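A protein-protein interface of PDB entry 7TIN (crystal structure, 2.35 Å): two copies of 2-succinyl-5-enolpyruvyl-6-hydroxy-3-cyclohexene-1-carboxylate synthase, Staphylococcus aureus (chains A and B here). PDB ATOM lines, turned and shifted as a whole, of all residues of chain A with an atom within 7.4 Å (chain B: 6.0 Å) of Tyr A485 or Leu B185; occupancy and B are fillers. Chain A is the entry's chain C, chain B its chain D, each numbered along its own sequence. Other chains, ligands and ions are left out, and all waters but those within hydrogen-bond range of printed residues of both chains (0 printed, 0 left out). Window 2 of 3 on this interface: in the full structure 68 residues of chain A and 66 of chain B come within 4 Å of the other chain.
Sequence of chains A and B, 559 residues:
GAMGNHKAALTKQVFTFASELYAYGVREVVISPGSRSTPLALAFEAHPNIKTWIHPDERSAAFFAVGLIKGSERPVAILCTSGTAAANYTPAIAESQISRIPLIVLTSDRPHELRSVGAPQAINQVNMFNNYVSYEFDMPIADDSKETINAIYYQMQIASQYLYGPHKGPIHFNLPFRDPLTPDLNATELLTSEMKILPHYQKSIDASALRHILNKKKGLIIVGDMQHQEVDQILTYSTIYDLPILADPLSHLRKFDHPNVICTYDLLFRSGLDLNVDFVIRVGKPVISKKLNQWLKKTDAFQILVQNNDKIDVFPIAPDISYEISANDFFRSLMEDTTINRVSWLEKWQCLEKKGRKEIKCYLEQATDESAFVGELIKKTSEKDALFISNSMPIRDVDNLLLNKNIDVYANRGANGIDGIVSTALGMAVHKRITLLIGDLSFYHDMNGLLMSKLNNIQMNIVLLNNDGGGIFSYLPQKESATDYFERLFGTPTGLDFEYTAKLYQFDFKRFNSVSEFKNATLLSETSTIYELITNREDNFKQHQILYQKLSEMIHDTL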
ATOM      1  N   GLN A 478      18.645 -28.542  -2.533  1.00  0.00           N
ATOM      2  CA  GLN A 478      18.503 -27.558  -1.463  1.00  0.00           C
ATOM      3  C   GLN A 478      18.922 -26.159  -1.893  1.00  0.00           C
ATOM      4  O   GLN A 478      18.575 -25.188  -1.213  1.00  0.00           O
ATOM      5  CB  GLN A 478      19.311 -27.988  -0.236  1.00  0.00           C
ATOM      6  CG  GLN A 478      18.816 -29.272   0.411  1.00  0.00           C
ATOM      7  CD  GLN A 478      19.382 -30.511  -0.253  1.00  0.00           C
ATOM      8  OE1 GLN A 478      19.185 -30.733  -1.448  1.00  0.00           O
ATOM      9  NE2 GLN A 478      20.087 -31.330   0.520  1.00  0.00           N
ATOM     10  N   SER A 481      15.218 -25.253  -2.890  1.00  0.00           N
ATOM     11  CA  SER A 481      14.185 -25.466  -1.884  1.00  0.00           C
ATOM     12  C   SER A 481      14.568 -24.925  -0.513  1.00  0.00           C
ATOM     13  O   SER A 481      13.749 -24.980   0.410  1.00  0.00           O
ATOM     14  CB  SER A 481      13.851 -26.958  -1.773  1.00  0.00           C
ATOM     15  OG  SER A 481      14.993 -27.720  -1.424  1.00  0.00           O
ATOM     16  N   ALA A 482      15.784 -24.412  -0.357  1.00  0.00           N
ATOM     17  CA  ALA A 482      16.211 -23.798   0.896  1.00  0.00           C
ATOM     18  C   ALA A 482      17.146 -22.629   0.592  1.00  0.00           C
ATOM     19  O   ALA A 482      18.199 -22.466   1.211  1.00  0.00           O
ATOM     20  CB  ALA A 482      16.871 -24.826   1.812  1.00  0.00           C
ATOM     21  N   THR A 483      16.750 -21.795  -0.375  1.00  0.00           N
ATOM     22  CA  THR A 483      17.579 -20.672  -0.812  1.00  0.00           C
ATOM     23  C   THR A 483      17.994 -19.781   0.355  1.00  0.00           C
ATOM     24  O   THR A 483      19.148 -19.343   0.432  1.00  0.00           O
ATOM     25  CB  THR A 483      16.824 -19.849  -1.859  1.00  0.00           C
ATOM     26  OG1 THR A 483      16.396 -20.702  -2.928  1.00  0.00           O
ATOM     27  CG2 THR A 483      17.712 -18.744  -2.418  1.00  0.00           C
ATOM     28  N   ASP A 484      17.068 -19.511   1.279  1.00  0.00           N
ATOM     29  CA  ASP A 484      17.350 -18.584   2.370  1.00  0.00           C
ATOM     30  C   ASP A 484      18.405 -19.109   3.335  1.00  0.00           C
ATOM     31  O   ASP A 484      19.005 -18.313   4.065  1.00  0.00           O
ATOM     32  CB  ASP A 484      16.062 -18.265   3.131  1.00  0.00           C
ATOM     33  CG  ASP A 484      15.112 -17.389   2.332  1.00  0.00           C
ATOM     34  OD1 ASP A 484      15.309 -17.254   1.104  1.00  0.00           O
ATOM     35  OD2 ASP A 484      14.165 -16.839   2.933  1.00  0.00           O
ATOM     36  N   TYR A 485      18.651 -20.419   3.359  1.00  0.00           N
ATOM     37  CA  TYR A 485      19.622 -21.012   4.268  1.00  0.00           C
ATOM     38  C   TYR A 485      20.817 -21.622   3.554  1.00  0.00           C
ATOM     39  O   TYR A 485      21.687 -22.198   4.215  1.00  0.00           O
ATOM     40  CB  TYR A 485      18.955 -22.092   5.127  1.00  0.00           C
ATOM     41  CG  TYR A 485      17.848 -21.597   6.033  1.00  0.00           C
ATOM     42  CD1 TYR A 485      18.136 -20.910   7.203  1.00  0.00           C
ATOM     43  CD2 TYR A 485      16.513 -21.837   5.724  1.00  0.00           C
ATOM     44  CE1 TYR A 485      17.127 -20.464   8.035  1.00  0.00           C
ATOM     45  CE2 TYR A 485      15.498 -21.398   6.550  1.00  0.00           C
ATOM     46  CZ  TYR A 485      15.810 -20.711   7.704  1.00  0.00           C
ATOM     47  OH  TYR A 485      14.802 -20.269   8.529  1.00  0.00           O
ATOM     48  N   PHE A 486      20.892 -21.506   2.227  1.00  0.00           N
ATOM     49  CA  PHE A 486      21.879 -22.271   1.473  1.00  0.00           C
ATOM     50  C   PHE A 486      23.303 -21.846   1.815  1.00  0.00           C
ATOM     51  O   PHE A 486      24.148 -22.687   2.136  1.00  0.00           O
ATOM     52  CB  PHE A 486      21.623 -22.125  -0.027  1.00  0.00           C
ATOM     53  CG  PHE A 486      22.623 -22.846  -0.873  1.00  0.00           C
ATOM     54  CD1 PHE A 486      22.500 -24.205  -1.102  1.00  0.00           C
ATOM     55  CD2 PHE A 486      23.702 -22.171  -1.419  1.00  0.00           C
ATOM     56  CE1 PHE A 486      23.425 -24.879  -1.874  1.00  0.00           C
ATOM     57  CE2 PHE A 486      24.636 -22.838  -2.190  1.00  0.00           C
ATOM     58  CZ  PHE A 486      24.495 -24.193  -2.421  1.00  0.00           C
ATOM     59  N   GLU A 487      23.590 -20.544   1.739  1.00  0.00           N
ATOM     60  CA  GLU A 487      24.960 -20.080   1.928  1.00  0.00           C
ATOM     61  C   GLU A 487      25.460 -20.275   3.352  1.00  0.00           C
ATOM     62  O   GLU A 487      26.675 -20.367   3.558  1.00  0.00           O
ATOM     63  CB  GLU A 487      25.083 -18.606   1.536  1.00  0.00           C
ATOM     64  CG  GLU A 487      25.053 -18.366   0.035  1.00  0.00           C
ATOM     65  CD  GLU A 487      26.169 -19.092  -0.694  1.00  0.00           C
ATOM     66  OE1 GLU A 487      27.345 -18.913  -0.308  1.00  0.00           O
ATOM     67  OE2 GLU A 487      25.874 -19.836  -1.657  1.00  0.00           O
ATOM     68  N   ARG A 488      24.567 -20.342   4.336  1.00  0.00           N
ATOM     69  CA  ARG A 488      25.020 -20.566   5.704  1.00  0.00           C
ATOM     70  C   ARG A 488      25.288 -22.043   5.970  1.00  0.00           C
ATOM     71  O   ARG A 488      26.293 -22.388   6.603  1.00  0.00           O
ATOM     72  CB  ARG A 488      23.998 -20.021   6.703  1.00  0.00           C
ATOM     73  CG  ARG A 488      24.467 -20.111   8.152  1.00  0.00           C
ATOM     74  CD  ARG A 488      23.693 -19.175   9.075  1.00  0.00           C
ATOM     75  NE  ARG A 488      23.818 -19.568  10.475  1.00  0.00           N
ATOM     76  CZ  ARG A 488      24.904 -19.386  11.215  1.00  0.00           C
ATOM     77  NH1 ARG A 488      25.979 -18.787  10.730  1.00  0.00           N
ATOM     78  NH2 ARG A 488      24.910 -19.814  12.475  1.00  0.00           N
ATOM     79  N   LEU A 489      24.415 -22.929   5.488  1.00  0.00           N
ATOM     80  CA  LEU A 489      24.562 -24.355   5.768  1.00  0.00           C
ATOM     81  C   LEU A 489      25.415 -25.087   4.741  1.00  0.00           C
ATOM     82  O   LEU A 489      26.080 -26.069   5.090  1.00  0.00           O
ATOM     83  CB  LEU A 489      23.188 -25.023   5.850  1.00  0.00           C
ATOM     84  CG  LEU A 489      22.344 -24.650   7.071  1.00  0.00           C
ATOM     85  CD1 LEU A 489      21.035 -25.417   7.084  1.00  0.00           C
ATOM     86  CD2 LEU A 489      23.123 -24.880   8.359  1.00  0.00           C
ATOM     87  N   PHE A 490      25.419 -24.643   3.492  1.00  0.00           N
ATOM     88  CA  PHE A 490      26.092 -25.383   2.433  1.00  0.00           C
ATOM     89  C   PHE A 490      27.231 -24.617   1.783  1.00  0.00           C
ATOM     90  O   PHE A 490      28.239 -25.223   1.413  1.00  0.00           O
ATOM     91  CB  PHE A 490      25.072 -25.803   1.368  1.00  0.00           C
ATOM     92  CG  PHE A 490      23.922 -26.589   1.924  1.00  0.00           C
ATOM     93  CD1 PHE A 490      24.108 -27.890   2.363  1.00  0.00           C
ATOM     94  CD2 PHE A 490      22.665 -26.023   2.031  1.00  0.00           C
ATOM     95  CE1 PHE A 490      23.058 -28.617   2.885  1.00  0.00           C
ATOM     96  CE2 PHE A 490      21.606 -26.745   2.555  1.00  0.00           C
ATOM     97  CZ  PHE A 490      21.804 -28.044   2.983  1.00  0.00           C
ATOM     98  N   GLY A 491      27.103 -23.301   1.631  1.00  0.00           N
ATOM     99  CA  GLY A 491      28.186 -22.508   1.087  1.00  0.00           C
ATOM    100  C   GLY A 491      29.405 -22.513   1.988  1.00  0.00           C
ATOM    101  O   GLY A 491      30.497 -22.882   1.553  1.00  0.00           O
ATOM    102  N   LYS B   7       7.499 -36.215   3.193  1.00  0.00           N
ATOM    103  CA  LYS B   7       8.012 -34.908   3.590  1.00  0.00           C
ATOM    104  C   LYS B   7       7.447 -34.467   4.935  1.00  0.00           C
ATOM    105  O   LYS B   7       8.185 -33.949   5.782  1.00  0.00           O
ATOM    106  CB  LYS B   7       7.702 -33.869   2.512  1.00  0.00           C
ATOM    107  CG  LYS B   7       8.324 -32.504   2.785  1.00  0.00           C
ATOM    108  CD  LYS B   7       7.773 -31.433   1.863  1.00  0.00           C
ATOM    109  CE  LYS B   7       8.712 -30.238   1.793  1.00  0.00           C
ATOM    110  NZ  LYS B   7       8.044 -29.030   1.226  1.00  0.00           N
ATOM    111  N   THR B  11       9.519 -33.952   8.366  1.00  0.00           N
ATOM    112  CA  THR B  11       9.443 -32.653   9.027  1.00  0.00           C
ATOM    113  C   THR B  11       8.983 -32.793  10.471  1.00  0.00           C
ATOM    114  O   THR B  11       9.506 -32.118  11.365  1.00  0.00           O
ATOM    115  CB  THR B  11       8.507 -31.724   8.253  1.00  0.00           C
ATOM    116  OG1 THR B  11       8.955 -31.618   6.895  1.00  0.00           O
ATOM    117  CG2 THR B  11       8.483 -30.340   8.882  1.00  0.00           C
ATOM    118  N   PHE B  15      11.658 -31.629  13.501  1.00  0.00           N
ATOM    119  CA  PHE B  15      11.184 -30.455  14.227  1.00  0.00           C
ATOM    120  C   PHE B  15      10.828 -30.797  15.670  1.00  0.00           C
ATOM    121  O   PHE B  15      11.020 -29.967  16.567  1.00  0.00           O
ATOM    122  CB  PHE B  15       9.982 -29.835  13.512  1.00  0.00           C
ATOM    123  CG  PHE B  15      10.346 -29.022  12.295  1.00  0.00           C
ATOM    124  CD1 PHE B  15      11.581 -29.170  11.678  1.00  0.00           C
ATOM    125  CD2 PHE B  15       9.447 -28.112  11.763  1.00  0.00           C
ATOM    126  CE1 PHE B  15      11.912 -28.427  10.560  1.00  0.00           C
ATOM    127  CE2 PHE B  15       9.770 -27.364  10.643  1.00  0.00           C
ATOM    128  CZ  PHE B  15      11.002 -27.522  10.041  1.00  0.00           C
ATOM    129  N   LEU B  42      18.551 -27.950   9.011  1.00  0.00           N
ATOM    130  CA  LEU B  42      17.572 -26.899   8.763  1.00  0.00           C
ATOM    131  C   LEU B  42      16.633 -26.708   9.949  1.00  0.00           C
ATOM    132  O   LEU B  42      16.213 -25.578  10.226  1.00  0.00           O
ATOM    133  CB  LEU B  42      16.785 -27.216   7.493  1.00  0.00           C
ATOM    134  CG  LEU B  42      17.568 -26.962   6.201  1.00  0.00           C
ATOM    135  CD1 LEU B  42      17.016 -27.791   5.057  1.00  0.00           C
ATOM    136  CD2 LEU B  42      17.549 -25.484   5.852  1.00  0.00           C
ATOM    137  N   ALA B  43      16.297 -27.790  10.659  1.00  0.00           N
ATOM    138  CA  ALA B  43      15.496 -27.668  11.874  1.00  0.00           C
ATOM    139  C   ALA B  43      16.158 -26.730  12.878  1.00  0.00           C
ATOM    140  O   ALA B  43      15.511 -25.829  13.423  1.00  0.00           O
ATOM    141  CB  ALA B  43      15.268 -29.045  12.495  1.00  0.00           C
ATOM    142  N   GLU B  45      18.385 -24.426  12.297  1.00  0.00           N
ATOM    143  CA  GLU B  45      18.421 -23.065  11.769  1.00  0.00           C
ATOM    144  C   GLU B  45      17.052 -22.408  11.851  1.00  0.00           C
ATOM    145  O   GLU B  45      16.940 -21.237  12.234  1.00  0.00           O
ATOM    146  CB  GLU B  45      18.926 -23.068  10.327  1.00  0.00           C
ATOM    147  CG  GLU B  45      20.439 -23.100  10.195  1.00  0.00           C
ATOM    148  CD  GLU B  45      21.112 -21.851  10.738  1.00  0.00           C
ATOM    149  OE1 GLU B  45      20.427 -20.824  10.925  1.00  0.00           O
ATOM    150  OE2 GLU B  45      22.336 -21.904  10.990  1.00  0.00           O
ATOM    151  N   ALA B  46      15.996 -23.147  11.500  1.00  0.00           N
ATOM    152  CA  ALA B  46      14.655 -22.577  11.524  1.00  0.00           C
ATOM    153  C   ALA B  46      14.162 -22.340  12.947  1.00  0.00           C
ATOM    154  O   ALA B  46      13.367 -21.422  13.176  1.00  0.00           O
ATOM    155  CB  ALA B  46      13.688 -23.488  10.768  1.00  0.00           C
ATOM    156  N   THR B 182      14.818 -32.342   2.158  1.00  0.00           N
ATOM    157  CA  THR B 182      14.426 -30.993   2.554  1.00  0.00           C
ATOM    158  C   THR B 182      13.107 -31.029   3.316  1.00  0.00           C
ATOM    159  O   THR B 182      12.097 -31.480   2.763  1.00  0.00           O
ATOM    160  CB  THR B 182      14.294 -30.090   1.336  1.00  0.00           C
ATOM    161  OG1 THR B 182      15.473 -30.201   0.527  1.00  0.00           O
ATOM    162  CG2 THR B 182      14.123 -28.639   1.771  1.00  0.00           C
ATOM    163  N   PRO B 183      13.067 -30.574   4.564  1.00  0.00           N
ATOM    164  CA  PRO B 183      11.805 -30.535   5.305  1.00  0.00           C
ATOM    165  C   PRO B 183      10.972 -29.318   4.918  1.00  0.00           C
ATOM    166  O   PRO B 183      11.413 -28.427   4.192  1.00  0.00           O
ATOM    167  CB  PRO B 183      12.270 -30.455   6.761  1.00  0.00           C
ATOM    168  CG  PRO B 183      13.528 -29.679   6.675  1.00  0.00           C
ATOM    169  CD  PRO B 183      14.202 -30.149   5.403  1.00  0.00           C
ATOM    170  N   ASP B 184       9.742 -29.298   5.431  1.00  0.00           N
ATOM    171  CA  ASP B 184       8.807 -28.202   5.190  1.00  0.00           C
ATOM    172  C   ASP B 184       9.086 -27.078   6.181  1.00  0.00           C
ATOM    173  O   ASP B 184       8.708 -27.166   7.354  1.00  0.00           O
ATOM    174  CB  ASP B 184       7.368 -28.698   5.317  1.00  0.00           C
ATOM    175  CG  ASP B 184       6.341 -27.589   5.134  1.00  0.00           C
ATOM    176  OD1 ASP B 184       6.695 -26.503   4.623  1.00  0.00           O
ATOM    177  OD2 ASP B 184       5.169 -27.810   5.509  1.00  0.00           O
ATOM    178  N   LEU B 185       9.725 -26.010   5.709  1.00  0.00           N
ATOM    179  CA  LEU B 185      10.052 -24.872   6.559  1.00  0.00           C
ATOM    180  C   LEU B 185       8.843 -24.005   6.889  1.00  0.00           C
ATOM    181  O   LEU B 185       9.011 -22.962   7.531  1.00  0.00           O
ATOM    182  CB  LEU B 185      11.140 -24.021   5.897  1.00  0.00           C
ATOM    183  CG  LEU B 185      12.360 -24.808   5.408  1.00  0.00           C
ATOM    184  CD1 LEU B 185      13.307 -23.919   4.623  1.00  0.00           C
ATOM    185  CD2 LEU B 185      13.081 -25.459   6.583  1.00  0.00           C
ATOM    186  N   ASN B 186       7.642 -24.402   6.467  1.00  0.00           N
ATOM    187  CA  ASN B 186       6.413 -23.716   6.842  1.00  0.00           C
ATOM    188  C   ASN B 186       5.733 -24.337   8.054  1.00  0.00           C
ATOM    189  O   ASN B 186       4.816 -23.724   8.611  1.00  0.00           O
ATOM    190  CB  ASN B 186       5.428 -23.697   5.665  1.00  0.00           C
ATOM    191  CG  ASN B 186       5.922 -22.854   4.504  1.00  0.00           C
ATOM    192  OD1 ASN B 186       6.728 -21.940   4.681  1.00  0.00           O
ATOM    193  ND2 ASN B 186       5.439 -23.158   3.308  1.00  0.00           N
ATOM    194  N   ALA B 187       6.157 -25.527   8.477  1.00  0.00           N
ATOM    195  CA  ALA B 187       5.596 -26.164   9.661  1.00  0.00           C
ATOM    196  C   ALA B 187       6.198 -25.569  10.930  1.00  0.00           C
ATOM    197  O   ALA B 187       6.616 -26.303  11.831  1.00  0.00           O
ATOM    198  CB  ALA B 187       5.828 -27.675   9.614  1.00  0.00           C
ATOM    199  N   THR B 188       6.232 -24.237  11.011  1.00  0.00           N
ATOM    200  CA  THR B 188       6.836 -23.558  12.151  1.00  0.00           C
ATOM    201  C   THR B 188       6.143 -23.892  13.467  1.00  0.00           C
ATOM    202  O   THR B 188       6.767 -23.774  14.529  1.00  0.00           O
ATOM    203  CB  THR B 188       6.811 -22.048  11.922  1.00  0.00           C
ATOM    204  OG1 THR B 188       5.483 -21.645  11.566  1.00  0.00           O
ATOM    205  CG2 THR B 188       7.763 -21.669  10.799  1.00  0.00           C
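Among the printed residues, merely in contact across the chains: Gln A478 with Thr B182, Tyr A485 with Leu B42, Tyr A485 with Glu B45, Tyr A485 with Ala B46, Tyr A485 with Leu B185, Leu A489 with Leu B42 and Leu A489 with Glu B45.
Of chain B, only Leu B42 (3.7 Å), Glu B45 (3.9 Å), Ala B46 (3.8 Å) and Leu B185 (3.9 Å) come within 4 Å of Tyr A485.
Leu B185 touches just one residue of chain A: Tyr A485 (3.9 Å).
Of the printed residues of chain B, Ser A481 touches Thr B182 (3.2 Å).
Printed residues of chain A within 4 Å of Ala B46: Tyr A485 (3.8 Å).
Of the printed residues of chain B, Gln A478 touches Thr B182.
Of the printed residues of chain B, Leu A489 touches Leu B42 (3.7 Å) and Glu B45 (3.7 Å).
Glu A487 touches none of the printed residues of chain B.
The nearest printed residue of chain A that does not touch Thr B182 is Ala A482 (4.7 Å).
Of the 14 printed residues of chain B, 5 touch a printed residue of chain A.
Hydrophobic or aromatic side chains of chain A that line the printed part of chain B: Tyr A485 and Leu A489.
Among the printed residues, Asp or Glu carboxylates within 4 Å of a Lys or Arg side-chain nitrogen of the other chain: Arg A488 with Glu B45 (2.8 Å).
The side-chain hydroxyl (OG) of Ser A481 lies within hydrogen-bond range of the side-chain hydroxyl (OG1) of Thr B182.
The side-chain carboxylate of Glu B45 lies within salt-bridge range of the guanidinium group of Arg A488.
No position is printed for both chains.
Of the 9 pairs that touch across the chains among the printed residues, none has its exchanged pair printed and touching as well.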
